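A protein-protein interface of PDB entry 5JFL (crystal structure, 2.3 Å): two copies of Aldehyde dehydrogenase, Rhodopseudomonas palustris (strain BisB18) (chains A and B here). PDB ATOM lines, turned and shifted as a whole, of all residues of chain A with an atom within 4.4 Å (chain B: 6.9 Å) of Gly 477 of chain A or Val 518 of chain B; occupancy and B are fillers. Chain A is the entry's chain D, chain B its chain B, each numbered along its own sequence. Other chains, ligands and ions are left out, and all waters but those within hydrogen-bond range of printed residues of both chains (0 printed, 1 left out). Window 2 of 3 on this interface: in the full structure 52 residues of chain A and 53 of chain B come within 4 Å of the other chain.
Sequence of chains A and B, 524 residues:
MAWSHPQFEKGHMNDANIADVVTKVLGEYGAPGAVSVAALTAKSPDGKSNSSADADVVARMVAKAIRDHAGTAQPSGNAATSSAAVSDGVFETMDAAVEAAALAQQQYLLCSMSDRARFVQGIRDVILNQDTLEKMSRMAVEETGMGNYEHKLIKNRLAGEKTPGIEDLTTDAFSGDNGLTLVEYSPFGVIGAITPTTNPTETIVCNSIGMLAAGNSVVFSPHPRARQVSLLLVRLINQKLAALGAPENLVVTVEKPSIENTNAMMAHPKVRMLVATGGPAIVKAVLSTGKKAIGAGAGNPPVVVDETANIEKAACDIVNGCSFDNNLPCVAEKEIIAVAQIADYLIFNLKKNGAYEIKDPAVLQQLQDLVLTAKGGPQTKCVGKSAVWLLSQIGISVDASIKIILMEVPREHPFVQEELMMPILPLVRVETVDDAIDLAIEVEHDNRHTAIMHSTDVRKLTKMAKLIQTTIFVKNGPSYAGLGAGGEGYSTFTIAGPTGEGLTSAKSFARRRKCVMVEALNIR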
ATOM      1  N   LYS A 313     -19.085  35.221  38.770  1.00  0.00           N
ATOM      2  CA  LYS A 313     -19.092  35.100  37.318  1.00  0.00           C
ATOM      3  C   LYS A 313     -20.305  35.796  36.714  1.00  0.00           C
ATOM      4  O   LYS A 313     -20.223  36.357  35.615  1.00  0.00           O
ATOM      5  CB  LYS A 313     -19.067  33.624  36.922  1.00  0.00           C
ATOM      6  CG  LYS A 313     -18.962  33.378  35.431  1.00  0.00           C
ATOM      7  CD  LYS A 313     -18.999  31.892  35.119  1.00  0.00           C
ATOM      8  CE  LYS A 313     -18.704  31.646  33.651  1.00  0.00           C
ATOM      9  NZ  LYS A 313     -19.576  32.479  32.776  1.00  0.00           N
ATOM     10  N   ASP A 317     -20.023  38.613  33.709  1.00  0.00           N
ATOM     11  CA  ASP A 317     -20.661  38.387  32.418  1.00  0.00           C
ATOM     12  C   ASP A 317     -21.680  39.475  32.104  1.00  0.00           C
ATOM     13  O   ASP A 317     -21.786  39.921  30.956  1.00  0.00           O
ATOM     14  CB  ASP A 317     -21.325  37.009  32.397  1.00  0.00           C
ATOM     15  CG  ASP A 317     -20.331  35.879  32.569  1.00  0.00           C
ATOM     16  OD1 ASP A 317     -19.127  36.102  32.325  1.00  0.00           O
ATOM     17  OD2 ASP A 317     -20.751  34.767  32.946  1.00  0.00           O
ATOM     18  N   ILE A 452     -31.424  35.981  28.987  1.00  0.00           N
ATOM     19  CA  ILE A 452     -30.269  35.403  29.659  1.00  0.00           C
ATOM     20  C   ILE A 452     -30.672  35.040  31.079  1.00  0.00           C
ATOM     21  O   ILE A 452     -31.513  35.702  31.695  1.00  0.00           O
ATOM     22  CB  ILE A 452     -29.053  36.361  29.665  1.00  0.00           C
ATOM     23  CG1 ILE A 452     -28.805  36.944  28.273  1.00  0.00           C
ATOM     24  CG2 ILE A 452     -27.799  35.646  30.151  1.00  0.00           C
ATOM     25  CD1 ILE A 452     -29.339  38.347  28.090  1.00  0.00           C
ATOM     26  N   HIS A 454     -28.461  33.522  34.612  1.00  0.00           N
ATOM     27  CA  HIS A 454     -27.379  32.888  35.348  1.00  0.00           C
ATOM     28  C   HIS A 454     -27.989  32.031  36.447  1.00  0.00           C
ATOM     29  O   HIS A 454     -28.658  32.546  37.350  1.00  0.00           O
ATOM     30  CB  HIS A 454     -26.422  33.931  35.917  1.00  0.00           C
ATOM     31  CG  HIS A 454     -25.719  34.723  34.862  1.00  0.00           C
ATOM     32  ND1 HIS A 454     -24.498  34.351  34.342  1.00  0.00           N
ATOM     33  CD2 HIS A 454     -26.080  35.850  34.206  1.00  0.00           C
ATOM     34  CE1 HIS A 454     -24.132  35.223  33.421  1.00  0.00           C
ATOM     35  NE2 HIS A 454     -25.074  36.144  33.319  1.00  0.00           N
ATOM     36  N   VAL A 474     -29.361  32.390  26.631  1.00  0.00           N
ATOM     37  CA  VAL A 474     -27.989  32.188  27.083  1.00  0.00           C
ATOM     38  C   VAL A 474     -28.002  31.829  28.562  1.00  0.00           C
ATOM     39  O   VAL A 474     -28.763  32.408  29.346  1.00  0.00           O
ATOM     40  CB  VAL A 474     -27.126  33.438  26.824  1.00  0.00           C
ATOM     41  CG1 VAL A 474     -25.681  33.186  27.223  1.00  0.00           C
ATOM     42  CG2 VAL A 474     -27.215  33.847  25.361  1.00  0.00           C
ATOM     43  N   LYS A 475     -27.151  30.875  28.940  1.00  0.00           N
ATOM     44  CA  LYS A 475     -27.054  30.391  30.311  1.00  0.00           C
ATOM     45  C   LYS A 475     -25.635  30.587  30.817  1.00  0.00           C
ATOM     46  O   LYS A 475     -24.683  30.121  30.183  1.00  0.00           O
ATOM     47  CB  LYS A 475     -27.426  28.913  30.402  1.00  0.00           C
ATOM     48  CG  LYS A 475     -28.878  28.632  30.167  1.00  0.00           C
ATOM     49  CD  LYS A 475     -29.059  27.183  29.830  1.00  0.00           C
ATOM     50  CE  LYS A 475     -30.348  26.974  29.105  1.00  0.00           C
ATOM     51  NZ  LYS A 475     -30.028  26.579  27.729  1.00  0.00           N
ATOM     52  N   ASN A 476     -25.498  31.261  31.959  1.00  0.00           N
ATOM     53  CA  ASN A 476     -24.231  31.332  32.689  1.00  0.00           C
ATOM     54  C   ASN A 476     -23.101  31.874  31.815  1.00  0.00           C
ATOM     55  O   ASN A 476     -21.979  31.364  31.830  1.00  0.00           O
ATOM     56  CB  ASN A 476     -23.865  29.965  33.269  1.00  0.00           C
ATOM     57  CG  ASN A 476     -24.878  29.477  34.285  1.00  0.00           C
ATOM     58  OD1 ASN A 476     -25.376  30.253  35.099  1.00  0.00           O
ATOM     59  ND2 ASN A 476     -25.196  28.188  34.235  1.00  0.00           N
ATOM     60  N   GLY A 477     -23.400  32.916  31.044  1.00  0.00           N
ATOM     61  CA  GLY A 477     -22.421  33.537  30.188  1.00  0.00           C
ATOM     62  C   GLY A 477     -22.844  34.928  29.767  1.00  0.00           C
ATOM     63  O   GLY A 477     -23.916  35.416  30.138  1.00  0.00           O
ATOM     64  N   PRO A 478     -21.996  35.605  28.999  1.00  0.00           N
ATOM     65  CA  PRO A 478     -22.367  36.915  28.462  1.00  0.00           C
ATOM     66  C   PRO A 478     -23.310  36.780  27.275  1.00  0.00           C
ATOM     67  O   PRO A 478     -23.384  35.742  26.615  1.00  0.00           O
ATOM     68  CB  PRO A 478     -21.024  37.525  28.033  1.00  0.00           C
ATOM     69  CG  PRO A 478     -19.964  36.637  28.643  1.00  0.00           C
ATOM     70  CD  PRO A 478     -20.586  35.284  28.732  1.00  0.00           C
ATOM     71  N   SER A 479     -24.035  37.869  27.012  1.00  0.00           N
ATOM     72  CA  SER A 479     -25.050  37.852  25.963  1.00  0.00           C
ATOM     73  C   SER A 479     -24.448  37.507  24.606  1.00  0.00           C
ATOM     74  O   SER A 479     -25.076  36.808  23.802  1.00  0.00           O
ATOM     75  CB  SER A 479     -25.760  39.203  25.903  1.00  0.00           C
ATOM     76  OG  SER A 479     -24.882  40.218  25.447  1.00  0.00           O
ATOM     77  N   ALA A 481     -22.509  35.379  23.780  1.00  0.00           N
ATOM     78  CA  ALA A 481     -22.343  33.953  23.527  1.00  0.00           C
ATOM     79  C   ALA A 481     -23.404  33.423  22.572  1.00  0.00           C
ATOM     80  O   ALA A 481     -23.200  32.371  21.957  1.00  0.00           O
ATOM     81  CB  ALA A 481     -22.379  33.171  24.839  1.00  0.00           C
ATOM     82  N   GLY A 486     -17.618  33.405  22.493  1.00  0.00           N
ATOM     83  CA  GLY A 486     -17.690  32.679  23.742  1.00  0.00           C
ATOM     84  C   GLY A 486     -18.816  31.676  23.811  1.00  0.00           C
ATOM     85  O   GLY A 486     -19.088  31.144  24.893  1.00  0.00           O
ATOM     86  N   ASP B 177     -15.524  23.927  23.654  1.00  0.00           N
ATOM     87  CA  ASP B 177     -14.964  24.608  24.818  1.00  0.00           C
ATOM     88  C   ASP B 177     -15.950  25.599  25.425  1.00  0.00           C
ATOM     89  O   ASP B 177     -16.022  25.733  26.652  1.00  0.00           O
ATOM     90  CB  ASP B 177     -13.661  25.312  24.442  1.00  0.00           C
ATOM     91  CG  ASP B 177     -12.589  24.341  24.017  1.00  0.00           C
ATOM     92  OD1 ASP B 177     -12.610  23.190  24.505  1.00  0.00           O
ATOM     93  OD2 ASP B 177     -11.728  24.721  23.196  1.00  0.00           O
ATOM     94  N   ASN B 178     -16.714  26.297  24.591  1.00  0.00           N
ATOM     95  CA  ASN B 178     -17.698  27.251  25.079  1.00  0.00           C
ATOM     96  C   ASN B 178     -18.997  26.587  25.515  1.00  0.00           C
ATOM     97  O   ASN B 178     -19.995  27.286  25.721  1.00  0.00           O
ATOM     98  CB  ASN B 178     -17.977  28.305  24.008  1.00  0.00           C
ATOM     99  CG  ASN B 178     -16.712  29.001  23.535  1.00  0.00           C
ATOM    100  OD1 ASN B 178     -16.501  29.188  22.337  1.00  0.00           O
ATOM    101  ND2 ASN B 178     -15.857  29.380  24.479  1.00  0.00           N
ATOM    102  N   GLY B 179     -19.009  25.262  25.654  1.00  0.00           N
ATOM    103  CA  GLY B 179     -20.154  24.572  26.212  1.00  0.00           C
ATOM    104  C   GLY B 179     -21.009  23.840  25.201  1.00  0.00           C
ATOM    105  O   GLY B 179     -20.493  23.183  24.293  1.00  0.00           O
ATOM    106  N   LEU B 180     -22.326  23.944  25.357  1.00  0.00           N
ATOM    107  CA  LEU B 180     -23.281  23.266  24.496  1.00  0.00           C
ATOM    108  C   LEU B 180     -24.264  24.277  23.925  1.00  0.00           C
ATOM    109  O   LEU B 180     -24.678  25.213  24.615  1.00  0.00           O
ATOM    110  CB  LEU B 180     -24.045  22.173  25.257  1.00  0.00           C
ATOM    111  CG  LEU B 180     -25.224  21.526  24.523  1.00  0.00           C
ATOM    112  CD1 LEU B 180     -24.745  20.763  23.296  1.00  0.00           C
ATOM    113  CD2 LEU B 180     -26.022  20.624  25.452  1.00  0.00           C
ATOM    114  N   VAL B 516     -28.093  28.257  24.521  1.00  0.00           N
ATOM    115  CA  VAL B 516     -26.643  28.238  24.687  1.00  0.00           C
ATOM    116  C   VAL B 516     -26.323  27.967  26.150  1.00  0.00           C
ATOM    117  O   VAL B 516     -26.598  28.801  27.021  1.00  0.00           O
ATOM    118  CB  VAL B 516     -26.005  29.553  24.224  1.00  0.00           C
ATOM    119  CG1 VAL B 516     -24.500  29.506  24.416  1.00  0.00           C
ATOM    120  CG2 VAL B 516     -26.362  29.834  22.771  1.00  0.00           C
ATOM    121  N   MET B 517     -25.723  26.810  26.422  1.00  0.00           N
ATOM    122  CA  MET B 517     -25.238  26.456  27.756  1.00  0.00           C
ATOM    123  C   MET B 517     -23.745  26.760  27.805  1.00  0.00           C
ATOM    124  O   MET B 517     -22.919  25.937  27.398  1.00  0.00           O
ATOM    125  CB  MET B 517     -25.517  24.991  28.069  1.00  0.00           C
ATOM    126  CG  MET B 517     -25.098  24.584  29.469  1.00  0.00           C
ATOM    127  SD  MET B 517     -26.143  25.319  30.737  1.00  0.00           S
ATOM    128  CE  MET B 517     -27.546  24.208  30.691  1.00  0.00           C
ATOM    129  N   VAL B 518     -23.397  27.939  28.315  1.00  0.00           N
ATOM    130  CA  VAL B 518     -22.012  28.398  28.292  1.00  0.00           C
ATOM    131  C   VAL B 518     -21.174  27.543  29.234  1.00  0.00           C
ATOM    132  O   VAL B 518     -21.476  27.428  30.427  1.00  0.00           O
ATOM    133  CB  VAL B 518     -21.919  29.882  28.666  1.00  0.00           C
ATOM    134  CG1 VAL B 518     -20.472  30.278  28.909  1.00  0.00           C
ATOM    135  CG2 VAL B 518     -22.541  30.738  27.576  1.00  0.00           C
ATOM    136  N   GLU B 519     -20.118  26.931  28.690  1.00  0.00           N
ATOM    137  CA  GLU B 519     -19.082  26.255  29.472  1.00  0.00           C
ATOM    138  C   GLU B 519     -19.622  25.076  30.274  1.00  0.00           C
ATOM    139  O   GLU B 519     -19.095  24.750  31.340  1.00  0.00           O
ATOM    140  CB  GLU B 519     -18.367  27.234  30.407  1.00  0.00           C
ATOM    141  CG  GLU B 519     -17.420  28.193  29.720  1.00  0.00           C
ATOM    142  CD  GLU B 519     -16.709  29.094  30.707  1.00  0.00           C
ATOM    143  OE1 GLU B 519     -17.135  30.257  30.869  1.00  0.00           O
ATOM    144  OE2 GLU B 519     -15.733  28.632  31.334  1.00  0.00           O
ATOM    145  N   ALA B 520     -20.664  24.415  29.779  1.00  0.00           N
ATOM    146  CA  ALA B 520     -21.212  23.272  30.491  1.00  0.00           C
ATOM    147  C   ALA B 520     -21.833  22.304  29.496  1.00  0.00           C
ATOM    148  O   ALA B 520     -22.189  22.675  28.374  1.00  0.00           O
ATOM    149  CB  ALA B 520     -22.242  23.701  31.544  1.00  0.00           C
ATOM    150  N   LEU B 521     -21.950  21.049  29.932  1.00  0.00           N
ATOM    151  CA  LEU B 521     -22.555  19.972  29.149  1.00  0.00           C
ATOM    152  C   LEU B 521     -21.790  19.706  27.858  1.00  0.00           C
ATOM    153  O   LEU B 521     -22.374  19.307  26.847  1.00  0.00           O
ATOM    154  CB  LEU B 521     -24.025  20.265  28.854  1.00  0.00           C
ATOM    155  CG  LEU B 521     -24.849  20.463  30.122  1.00  0.00           C
ATOM    156  CD1 LEU B 521     -26.173  21.057  29.757  1.00  0.00           C
ATOM    157  CD2 LEU B 521     -25.034  19.147  30.859  1.00  0.00           C
ATOM    158  N   ASN B 522     -20.479  19.927  27.886  1.00  0.00           N
ATOM    159  CA  ASN B 522     -19.584  19.577  26.787  1.00  0.00           C
ATOM    160  C   ASN B 522     -18.798  18.345  27.233  1.00  0.00           C
ATOM    161  O   ASN B 522     -17.657  18.431  27.688  1.00  0.00           O
ATOM    162  CB  ASN B 522     -18.672  20.752  26.424  1.00  0.00           C
ATOM    163  CG  ASN B 522     -18.033  21.401  27.640  1.00  0.00           C
ATOM    164  OD1 ASN B 522     -18.651  21.515  28.697  1.00  0.00           O
ATOM    165  ND2 ASN B 522     -16.787  21.833  27.491  1.00  0.00           N
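No position is printed for both chains. Of the 11 pairs that touch across the chains among the printed residues, none has its exchanged pair printed and touching as well.
Of chain B, only Val 518 (3.8 Å) comes within 4 Å of Gly 477 of chain A. Of the printed residues of chain A, Val 518 of chain B touches Val 474, Lys 475, Asn 476, Gly 477 and Ala 481. Printed residues of chain A within 4 Å of Val 516 of chain B: Val 474 (3.7 Å), Lys 475 (2.9 Å) and Ala 481 (3.99 Å). Printed residues of chain A within 4 Å of Glu 519 of chain B: Lys 313 (3.5 Å).
Of the 12 printed residues of chain A, 7 touch a printed residue of chain B. Hydrophobic or aromatic side chains of chain A that line the printed part of chain B: Val 474 and Ala 481. Of the 11 printed residues of chain B, 5 touch a printed residue of chain A. Among the printed residues, Asp or Glu carboxylates within 4 Å of a Lys or Arg side-chain nitrogen of the other chain: Lys 313 of chain A with Glu 519 of chain B.
O of Asn 178 of chain B lies within hydrogen-bond range of N of Glu 519 of chain B (3.0 Å). The backbone carbonyl oxygen (O) of Leu 180 of chain B lies within hydrogen-bond range of the backbone NH (N) of Met 517 of chain B, at 2.6 Å. NZ of Lys 313 of chain A is in salt-bridge range of OD2 of Asp 317 of chain A (2.6 Å). NZ of Lys 313 of chain A sits at hydrogen-bond distance from O of Asn 476 of chain A (2.8 Å). The backbone carbonyl oxygen of Gly 477 of chain A lies close to a ring nitrogen (NE2) of His 454 of chain A, at 3.5 Å.
Among the printed residues, merely in contact across the chains: Gly 486 of chain A with Asn 178 of chain B, Lys 475 of chain A with Met 517 of chain B, Asn 476 of chain A with Val 518 of chain B, Val 474 of chain A with Val 516 of chain B, Ala 481 of chain A with Val 518 of chain B, Gly 477 of chain A with Val 518 of chain B, Ala 481 of chain A with Val 516 of chain B and Val 474 of chain A with Val 518 of chain B.
The backbone NH of Lys 475 of chain A is in hydrogen-bond range of the backbone carbonyl oxygen of Val 516 of chain B (2.9 Å). N of Val 518 of chain B sits at hydrogen-bond distance from O of Lys 475 of chain A (3.1 Å). The side-chain carboxylate of Glu 519 of chain B is in salt-bridge range of the side-chain amino group of Lys 313 of chain A (3.8 Å).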
